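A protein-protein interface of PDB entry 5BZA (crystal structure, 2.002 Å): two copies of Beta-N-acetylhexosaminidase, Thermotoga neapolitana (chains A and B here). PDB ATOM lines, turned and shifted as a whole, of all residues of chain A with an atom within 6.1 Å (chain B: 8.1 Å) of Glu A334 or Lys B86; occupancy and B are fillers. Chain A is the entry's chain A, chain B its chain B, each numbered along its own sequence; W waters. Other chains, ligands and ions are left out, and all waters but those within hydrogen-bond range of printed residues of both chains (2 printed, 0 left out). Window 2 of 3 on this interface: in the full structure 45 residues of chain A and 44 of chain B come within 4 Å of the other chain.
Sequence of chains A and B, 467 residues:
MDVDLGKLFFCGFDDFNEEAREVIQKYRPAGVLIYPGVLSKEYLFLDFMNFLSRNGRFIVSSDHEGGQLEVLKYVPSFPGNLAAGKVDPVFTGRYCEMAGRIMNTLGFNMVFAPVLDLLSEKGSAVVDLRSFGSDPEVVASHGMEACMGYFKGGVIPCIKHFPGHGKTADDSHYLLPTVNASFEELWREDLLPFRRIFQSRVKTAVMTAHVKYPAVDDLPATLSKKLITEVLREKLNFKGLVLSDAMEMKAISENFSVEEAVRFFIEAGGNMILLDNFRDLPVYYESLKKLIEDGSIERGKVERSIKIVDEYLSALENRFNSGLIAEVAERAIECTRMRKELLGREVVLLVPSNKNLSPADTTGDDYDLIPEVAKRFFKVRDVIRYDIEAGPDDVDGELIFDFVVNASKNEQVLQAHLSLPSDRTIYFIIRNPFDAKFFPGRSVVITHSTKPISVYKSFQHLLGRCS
The side-chain amino group of Lys B86 lies within salt-bridge range of the side-chain carboxylate of Glu A334 (3.3 Å).
The backbone carbonyl oxygen of Val B87 sits at hydrogen-bond distance from a ring nitrogen (NE2) of His B142 (2.5 Å). The side-chain sulfur of Cys A335 is disulfide-bonded to the side-chain sulfur of Cys A466 (2.0 Å). The side-chain carboxylate (OE2) of Glu A334 sits close to a ring nitrogen (NE2) of His A448 (3.5 Å). The backbone carbonyl oxygen (O) of Glu A334 sits at hydrogen-bond distance from the backbone NH (N) of Ile A446, 2.7 Å away. N of Leu B82 sits close to O of Ser B131 (3.2 Å). The backbone carbonyl oxygen of Ala A332 is in hydrogen-bond range of a ring nitrogen (ND1) of His A448, at 2.5 Å.
Val B87 touches Arg A331 (CG2 to CB, 3.7 Å). Ala B83 touches Ala A332 (O to CB, 3.5 Å). Ala A332 touches Val B87. O of His A448 touches CB of Leu B82, at 3.9 Å. Ala B83 touches His A448. Lys B86 touches His A448 (CG to NE2, 3.6 Å).
Of the printed residues of chain B, Arg A331 touches Val B87 (3.7 Å). Of chain B, only Lys B86 comes within 4 Å of Glu A334. Printed residues of chain A within 4 Å of Leu B82: His A448 (3.9 Å). Lys B86 touches just these residues of chain A: Glu A334 and His A448. Of the printed residues of chain A, Val B87 touches Arg A331 (3.7 Å) and Ala A332 (3.8 Å). The nearest residue of chain A that does not touch Lys B86 is Ala A332 (4.1 Å).
Of the 16 printed residues of chain B, 4 touch a printed residue of chain A. Hydrophobic or aromatic side chains of chain B that line the printed part of chain A: Leu B82, Ala B83 and Val B87. Hydrophobic or aromatic side chains of chain A within 4 Å of the printed part of chain B: Ala A332 and His A448. Among the printed residues, 7 pairs touch across the chains.
No position is printed for both chains. Of the 7 pairs that touch across the chains among the printed residues, none has its exchanged pair printed and touching as well.
Water W1 lies within hydrogen-bond range of NH2 of Arg A331 and OD2 of Asp B88. Water W2 lies within hydrogen-bond range of O of His A448 (3.1 Å), N of Leu B82 (3.3 Å), N of Ala B83 (3.3 Å) and O of Gly B80 (3.4 Å).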
ATOM      1  N   ARG A 331      16.584   6.558 -19.783  1.00  0.00           N
ATOM      2  CA  ARG A 331      17.721   5.804 -19.274  1.00  0.00           C
ATOM      3  C   ARG A 331      17.774   5.823 -17.726  1.00  0.00           C
ATOM      4  O   ARG A 331      18.488   5.036 -17.115  1.00  0.00           O
ATOM      5  CB  ARG A 331      18.999   6.342 -19.925  1.00  0.00           C
ATOM      6  CG  ARG A 331      19.283   5.701 -21.301  1.00  0.00           C
ATOM      7  CD  ARG A 331      19.995   6.659 -22.261  1.00  0.00           C
ATOM      8  NE  ARG A 331      21.440   6.601 -22.178  1.00  0.00           N
ATOM      9  CZ  ARG A 331      22.296   6.585 -23.209  1.00  0.00           C
ATOM     10  NH1 ARG A 331      21.894   6.663 -24.472  1.00  0.00           N
ATOM     11  NH2 ARG A 331      23.598   6.529 -22.933  1.00  0.00           N
ATOM     12  N   ALA A 332      16.973   6.684 -17.096  1.00  0.00           N
ATOM     13  CA  ALA A 332      16.934   6.754 -15.646  1.00  0.00           C
ATOM     14  C   ALA A 332      15.864   5.832 -15.028  1.00  0.00           C
ATOM     15  O   ALA A 332      15.594   5.899 -13.825  1.00  0.00           O
ATOM     16  CB  ALA A 332      16.699   8.186 -15.212  1.00  0.00           C
ATOM     17  N   ILE A 333      15.278   4.942 -15.819  1.00  0.00           N
ATOM     18  CA  ILE A 333      14.213   4.116 -15.273  1.00  0.00           C
ATOM     19  C   ILE A 333      14.675   2.710 -14.902  1.00  0.00           C
ATOM     20  O   ILE A 333      15.429   2.055 -15.631  1.00  0.00           O
ATOM     21  CB  ILE A 333      13.048   4.037 -16.243  1.00  0.00           C
ATOM     22  CG1 ILE A 333      12.113   5.223 -15.972  1.00  0.00           C
ATOM     23  CG2 ILE A 333      12.317   2.714 -16.104  1.00  0.00           C
ATOM     24  CD1 ILE A 333      11.391   5.499 -17.111  1.00  0.00           C
ATOM     25  N   GLU A 334      14.265   2.258 -13.727  1.00  0.00           N
ATOM     26  CA  GLU A 334      14.632   0.913 -13.330  1.00  0.00           C
ATOM     27  C   GLU A 334      13.402   0.086 -12.995  1.00  0.00           C
ATOM     28  O   GLU A 334      12.395   0.586 -12.439  1.00  0.00           O
ATOM     29  CB  GLU A 334      15.606   0.942 -12.151  1.00  0.00           C
ATOM     30  CG  GLU A 334      16.668   1.982 -12.305  1.00  0.00           C
ATOM     31  CD  GLU A 334      17.758   1.833 -11.267  1.00  0.00           C
ATOM     32  OE1 GLU A 334      18.536   0.868 -11.414  1.00  0.00           O
ATOM     33  OE2 GLU A 334      17.849   2.655 -10.320  1.00  0.00           O
ATOM     34  N   CYS A 335      13.459  -1.172 -13.390  1.00  0.00           N
ATOM     35  CA  CYS A 335      12.344  -2.048 -13.107  1.00  0.00           C
ATOM     36  C   CYS A 335      12.806  -3.430 -12.700  1.00  0.00           C
ATOM     37  O   CYS A 335      13.802  -3.951 -13.222  1.00  0.00           O
ATOM     38  CB  CYS A 335      11.412  -2.142 -14.321  1.00  0.00           C
ATOM     39  SG  CYS A 335      12.241  -2.818 -15.774  1.00  0.00           S
ATOM     40  N   THR A 336      12.065  -4.013 -11.759  1.00  0.00           N
ATOM     41  CA  THR A 336      12.071  -5.459 -11.548  1.00  0.00           C
ATOM     42  C   THR A 336      11.413  -6.139 -12.749  1.00  0.00           C
ATOM     43  O   THR A 336      10.764  -5.465 -13.579  1.00  0.00           O
ATOM     44  CB  THR A 336      11.302  -5.848 -10.278  1.00  0.00           C
ATOM     45  OG1 THR A 336       9.933  -5.405 -10.384  1.00  0.00           O
ATOM     46  CG2 THR A 336      11.936  -5.198  -9.049  1.00  0.00           C
ATOM     47  N   VAL A 444       8.265  -3.361  -8.814  1.00  0.00           N
ATOM     48  CA  VAL A 444       8.690  -2.009  -8.495  1.00  0.00           C
ATOM     49  C   VAL A 444       9.271  -1.355  -9.740  1.00  0.00           C
ATOM     50  O   VAL A 444      10.050  -1.981 -10.469  1.00  0.00           O
ATOM     51  CB  VAL A 444       9.779  -1.998  -7.336  1.00  0.00           C
ATOM     52  CG1 VAL A 444      10.362  -0.589  -7.154  1.00  0.00           C
ATOM     53  CG2 VAL A 444       9.208  -2.545  -5.981  1.00  0.00           C
ATOM     54  N   VAL A 445       8.875  -0.113  -9.989  1.00  0.00           N
ATOM     55  CA  VAL A 445       9.468   0.698 -11.064  1.00  0.00           C
ATOM     56  C   VAL A 445      10.041   1.971 -10.457  1.00  0.00           C
ATOM     57  O   VAL A 445       9.323   2.695  -9.763  1.00  0.00           O
ATOM     58  CB  VAL A 445       8.406   1.071 -12.175  1.00  0.00           C
ATOM     59  CG1 VAL A 445       8.892   2.228 -13.070  1.00  0.00           C
ATOM     60  CG2 VAL A 445       8.028  -0.147 -13.006  1.00  0.00           C
ATOM     61  N   ILE A 446      11.315   2.267 -10.697  1.00  0.00           N
ATOM     62  CA  ILE A 446      11.865   3.536 -10.191  1.00  0.00           C
ATOM     63  C   ILE A 446      12.130   4.502 -11.340  1.00  0.00           C
ATOM     64  O   ILE A 446      12.794   4.157 -12.321  1.00  0.00           O
ATOM     65  CB  ILE A 446      13.184   3.336  -9.351  1.00  0.00           C
ATOM     66  CG1 ILE A 446      12.980   2.278  -8.259  1.00  0.00           C
ATOM     67  CG2 ILE A 446      13.639   4.666  -8.709  1.00  0.00           C
ATOM     68  CD1 ILE A 446      14.299   1.961  -7.510  1.00  0.00           C
ATOM     69  N   THR A 447      11.601   5.711 -11.210  1.00  0.00           N
ATOM     70  CA  THR A 447      11.663   6.694 -12.287  1.00  0.00           C
ATOM     71  C   THR A 447      12.703   7.788 -12.039  1.00  0.00           C
ATOM     72  O   THR A 447      13.219   8.379 -12.978  1.00  0.00           O
ATOM     73  CB  THR A 447      10.288   7.357 -12.503  1.00  0.00           C
ATOM     74  OG1 THR A 447       9.894   8.025 -11.295  1.00  0.00           O
ATOM     75  CG2 THR A 447       9.241   6.299 -12.925  1.00  0.00           C
ATOM     76  N   HIS A 448      12.963   8.072 -10.768  1.00  0.00           N
ATOM     77  CA  HIS A 448      13.884   9.128 -10.352  1.00  0.00           C
ATOM     78  C   HIS A 448      13.378  10.508 -10.723  1.00  0.00           C
ATOM     79  O   HIS A 448      14.166  11.446 -10.761  1.00  0.00           O
ATOM     80  CB  HIS A 448      15.266   8.939 -10.951  1.00  0.00           C
ATOM     81  CG  HIS A 448      15.895   7.638 -10.604  1.00  0.00           C
ATOM     82  ND1 HIS A 448      15.903   6.560 -11.469  1.00  0.00           N
ATOM     83  CD2 HIS A 448      16.533   7.227  -9.483  1.00  0.00           C
ATOM     84  CE1 HIS A 448      16.544   5.552 -10.905  1.00  0.00           C
ATOM     85  NE2 HIS A 448      16.926   5.932  -9.703  1.00  0.00           N
ATOM     86  N   HIS A 461       8.676   1.472 -20.787  1.00  0.00           N
ATOM     87  CA  HIS A 461       9.594   0.489 -20.244  1.00  0.00           C
ATOM     88  C   HIS A 461       8.819  -0.773 -19.748  1.00  0.00           C
ATOM     89  O   HIS A 461       9.184  -1.881 -20.007  1.00  0.00           O
ATOM     90  CB  HIS A 461      10.467   1.119 -19.157  1.00  0.00           C
ATOM     91  CG  HIS A 461      11.902   1.242 -19.538  1.00  0.00           C
ATOM     92  ND1 HIS A 461      12.412   2.327 -20.192  1.00  0.00           N
ATOM     93  CD2 HIS A 461      12.945   0.406 -19.348  1.00  0.00           C
ATOM     94  CE1 HIS A 461      13.694   2.147 -20.418  1.00  0.00           C
ATOM     95  NE2 HIS A 461      14.040   0.977 -19.927  1.00  0.00           N
ATOM     96  N   ARG A 465      10.879  -3.090 -22.303  1.00  0.00           N
ATOM     97  CA  ARG A 465      12.070  -3.802 -21.867  1.00  0.00           C
ATOM     98  C   ARG A 465      11.880  -4.553 -20.514  1.00  0.00           C
ATOM     99  O   ARG A 465      12.488  -5.604 -20.308  1.00  0.00           O
ATOM    100  CB  ARG A 465      13.250  -2.817 -21.771  1.00  0.00           C
ATOM    101  CG  ARG A 465      14.170  -3.114 -20.601  1.00  0.00           C
ATOM    102  CD  ARG A 465      15.130  -1.990 -20.234  1.00  0.00           C
ATOM    103  NE  ARG A 465      15.896  -2.339 -19.031  1.00  0.00           N
ATOM    104  CZ  ARG A 465      15.569  -1.951 -17.799  1.00  0.00           C
ATOM    105  NH1 ARG A 465      14.482  -1.203 -17.610  1.00  0.00           N
ATOM    106  NH2 ARG A 465      16.317  -2.310 -16.755  1.00  0.00           N
ATOM    107  N   CYS A 466      11.047  -4.031 -19.605  1.00  0.00           N
ATOM    108  CA  CYS A 466      10.787  -4.692 -18.301  1.00  0.00           C
ATOM    109  C   CYS A 466       9.978  -6.000 -18.381  1.00  0.00           C
ATOM    110  O   CYS A 466       9.720  -6.638 -17.344  1.00  0.00           O
ATOM    111  CB  CYS A 466      10.057  -3.743 -17.346  1.00  0.00           C
ATOM    112  SG  CYS A 466      10.858  -2.152 -17.115  1.00  0.00           S
ATOM    113  N   GLY B  80      15.327  16.205 -14.074  1.00  0.00           N
ATOM    114  CA  GLY B  80      16.047  16.794 -12.960  1.00  0.00           C
ATOM    115  C   GLY B  80      17.345  16.092 -12.603  1.00  0.00           C
ATOM    116  O   GLY B  80      17.724  15.072 -13.190  1.00  0.00           O
ATOM    117  N   ASN B  81      18.064  16.659 -11.638  1.00  0.00           N
ATOM    118  CA  ASN B  81      19.401  16.132 -11.308  1.00  0.00           C
ATOM    119  C   ASN B  81      19.440  14.670 -10.904  1.00  0.00           C
ATOM    120  O   ASN B  81      20.378  13.967 -11.268  1.00  0.00           O
ATOM    121  CB  ASN B  81      20.053  16.983 -10.219  1.00  0.00           C
ATOM    122  CG  ASN B  81      20.719  18.222 -10.802  1.00  0.00           C
ATOM    123  OD1 ASN B  81      20.503  18.571 -11.974  1.00  0.00           O
ATOM    124  ND2 ASN B  81      21.533  18.885 -10.001  1.00  0.00           N
ATOM    125  N   LEU B  82      18.433  14.180 -10.205  1.00  0.00           N
ATOM    126  CA  LEU B  82      18.518  12.801  -9.730  1.00  0.00           C
ATOM    127  C   LEU B  82      18.496  11.814 -10.913  1.00  0.00           C
ATOM    128  O   LEU B  82      19.419  10.935 -11.074  1.00  0.00           O
ATOM    129  CB  LEU B  82      17.382  12.517  -8.740  1.00  0.00           C
ATOM    130  CG  LEU B  82      17.509  11.176  -8.020  1.00  0.00           C
ATOM    131  CD1 LEU B  82      18.739  11.163  -7.078  1.00  0.00           C
ATOM    132  CD2 LEU B  82      16.233  10.849  -7.262  1.00  0.00           C
ATOM    133  N   ALA B  83      17.488  12.006 -11.787  1.00  0.00           N
ATOM    134  CA  ALA B  83      17.413  11.223 -13.010  1.00  0.00           C
ATOM    135  C   ALA B  83      18.671  11.415 -13.809  1.00  0.00           C
ATOM    136  O   ALA B  83      19.249  10.436 -14.261  1.00  0.00           O
ATOM    137  CB  ALA B  83      16.204  11.611 -13.844  1.00  0.00           C
ATOM    138  N   ALA B  84      19.140  12.658 -13.914  1.00  0.00           N
ATOM    139  CA  ALA B  84      20.342  12.934 -14.708  1.00  0.00           C
ATOM    140  C   ALA B  84      21.555  12.151 -14.188  1.00  0.00           C
ATOM    141  O   ALA B  84      22.306  11.542 -14.963  1.00  0.00           O
ATOM    142  CB  ALA B  84      20.650  14.456 -14.709  1.00  0.00           C
ATOM    143  N   GLY B  85      21.720  12.149 -12.864  1.00  0.00           N
ATOM    144  CA  GLY B  85      22.807  11.450 -12.181  1.00  0.00           C
ATOM    145  C   GLY B  85      22.786   9.965 -12.484  1.00  0.00           C
ATOM    146  O   GLY B  85      23.823   9.293 -12.401  1.00  0.00           O
ATOM    147  N   LYS B  86      21.598   9.417 -12.779  1.00  0.00           N
ATOM    148  CA  LYS B  86      21.566   7.988 -13.149  1.00  0.00           C
ATOM    149  C   LYS B  86      22.142   7.686 -14.532  1.00  0.00           C
ATOM    150  O   LYS B  86      22.323   6.519 -14.881  1.00  0.00           O
ATOM    151  CB  LYS B  86      20.152   7.430 -13.085  1.00  0.00           C
ATOM    152  CG  LYS B  86      19.563   7.326 -11.674  1.00  0.00           C
ATOM    153  CD  LYS B  86      20.608   6.832 -10.627  1.00  0.00           C
ATOM    154  CE  LYS B  86      20.940   5.383 -10.863  1.00  0.00           C
ATOM    155  NZ  LYS B  86      20.542   4.496  -9.747  1.00  0.00           N
ATOM    156  N   VAL B  87      22.430   8.725 -15.314  1.00  0.00           N
ATOM    157  CA  VAL B  87      22.697   8.578 -16.736  1.00  0.00           C
ATOM    158  C   VAL B  87      24.058   9.184 -17.045  1.00  0.00           C
ATOM    159  O   VAL B  87      24.546  10.032 -16.287  1.00  0.00           O
ATOM    160  CB  VAL B  87      21.564   9.262 -17.556  1.00  0.00           C
ATOM    161  CG1 VAL B  87      21.831   9.229 -19.031  1.00  0.00           C
ATOM    162  CG2 VAL B  87      20.223   8.575 -17.236  1.00  0.00           C
ATOM    163  N   ASP B  88      24.667   8.740 -18.136  1.00  0.00           N
ATOM    164  CA  ASP B  88      25.847   9.373 -18.712  1.00  0.00           C
ATOM    165  C   ASP B  88      25.834  10.906 -18.597  1.00  0.00           C
ATOM    166  O   ASP B  88      24.959  11.574 -19.175  1.00  0.00           O
ATOM    167  CB  ASP B  88      25.939   9.001 -20.194  1.00  0.00           C
ATOM    168  CG  ASP B  88      27.263   9.409 -20.832  1.00  0.00           C
ATOM    169  OD1 ASP B  88      27.950  10.326 -20.347  1.00  0.00           O
ATOM    170  OD2 ASP B  88      27.596   8.816 -21.872  1.00  0.00           O
ATOM    171  N   PRO B  89      26.834  11.469 -17.884  1.00  0.00           N
ATOM    172  CA  PRO B  89      26.903  12.914 -17.623  1.00  0.00           C
ATOM    173  C   PRO B  89      26.868  13.792 -18.896  1.00  0.00           C
ATOM    174  O   PRO B  89      26.441  14.972 -18.847  1.00  0.00           O
ATOM    175  CB  PRO B  89      28.260  13.079 -16.886  1.00  0.00           C
ATOM    176  CG  PRO B  89      28.987  11.790 -17.084  1.00  0.00           C
ATOM    177  CD  PRO B  89      27.938  10.735 -17.232  1.00  0.00           C
ATOM    178  N   THR B  92      23.771  15.416 -19.291  1.00  0.00           N
ATOM    179  CA  THR B  92      23.610  16.605 -18.443  1.00  0.00           C
ATOM    180  C   THR B  92      24.223  17.869 -19.089  1.00  0.00           C
ATOM    181  O   THR B  92      23.630  18.971 -19.051  1.00  0.00           O
ATOM    182  CB  THR B  92      24.239  16.373 -17.032  1.00  0.00           C
ATOM    183  OG1 THR B  92      23.632  15.198 -16.446  1.00  0.00           O
ATOM    184  CG2 THR B  92      24.083  17.604 -16.149  1.00  0.00           C
ATOM    185  N   SER B 131      19.497  16.864  -6.390  1.00  0.00           N
ATOM    186  CA  SER B 131      20.881  16.414  -6.402  1.00  0.00           C
ATOM    187  C   SER B 131      21.156  15.309  -7.446  1.00  0.00           C
ATOM    188  O   SER B 131      20.366  14.391  -7.660  1.00  0.00           O
ATOM    189  CB  SER B 131      21.310  15.925  -4.974  1.00  0.00           C
ATOM    190  OG  SER B 131      22.518  15.155  -5.015  1.00  0.00           O
ATOM    191  N   PHE B 132      22.335  15.359  -8.031  1.00  0.00           N
ATOM    192  CA  PHE B 132      22.768  14.326  -8.945  1.00  0.00           C
ATOM    193  C   PHE B 132      22.905  12.967  -8.266  1.00  0.00           C
ATOM    194  O   PHE B 132      22.871  11.949  -8.958  1.00  0.00           O
ATOM    195  CB  PHE B 132      24.127  14.722  -9.567  1.00  0.00           C
ATOM    196  CG  PHE B 132      24.050  15.875 -10.544  1.00  0.00           C
ATOM    197  CD1 PHE B 132      23.358  15.735 -11.756  1.00  0.00           C
ATOM    198  CD2 PHE B 132      24.645  17.105 -10.238  1.00  0.00           C
ATOM    199  CE1 PHE B 132      23.287  16.789 -12.688  1.00  0.00           C
ATOM    200  CE2 PHE B 132      24.561  18.175 -11.150  1.00  0.00           C
ATOM    201  CZ  PHE B 132      23.873  17.999 -12.393  1.00  0.00           C
ATOM    202  N   GLY B 133      23.126  12.942  -6.933  1.00  0.00           N
ATOM    203  CA  GLY B 133      23.217  11.673  -6.199  1.00  0.00           C
ATOM    204  C   GLY B 133      24.064  11.665  -4.929  1.00  0.00           C
ATOM    205  O   GLY B 133      24.558  12.711  -4.523  1.00  0.00           O
ATOM    206  N   VAL B 138      30.065  10.833  -8.938  1.00  0.00           N
ATOM    207  CA  VAL B 138      28.954  10.972  -9.868  1.00  0.00           C
ATOM    208  C   VAL B 138      28.506  12.425  -9.909  1.00  0.00           C
ATOM    209  O   VAL B 138      28.268  13.006 -11.002  1.00  0.00           O
ATOM    210  CB  VAL B 138      27.767  10.041  -9.458  1.00  0.00           C
ATOM    211  CG1 VAL B 138      26.502  10.301 -10.334  1.00  0.00           C
ATOM    212  CG2 VAL B 138      28.195   8.583  -9.592  1.00  0.00           C
ATOM    213  N   HIS B 142      28.858  14.949 -13.281  1.00  0.00           N
ATOM    214  CA  HIS B 142      27.630  15.567 -13.774  1.00  0.00           C
ATOM    215  C   HIS B 142      27.633  17.085 -13.548  1.00  0.00           C
ATOM    216  O   HIS B 142      27.119  17.845 -14.372  1.00  0.00           O
ATOM    217  CB  HIS B 142      26.417  14.931 -13.124  1.00  0.00           C
ATOM    218  CG  HIS B 142      26.140  13.549 -13.616  1.00  0.00           C
ATOM    219  ND1 HIS B 142      26.883  12.450 -13.219  1.00  0.00           N
ATOM    220  CD2 HIS B 142      25.233  13.086 -14.508  1.00  0.00           C
ATOM    221  CE1 HIS B 142      26.405  11.369 -13.805  1.00  0.00           C
ATOM    222  NE2 HIS B 142      25.411  11.728 -14.606  1.00  0.00           N
HETATM  223  O   HOH W   1      26.004   6.866 -23.661  1.00  0.00           O
HETATM  224  O   HOH W   2      15.261  14.293 -10.999  1.00  0.00           O
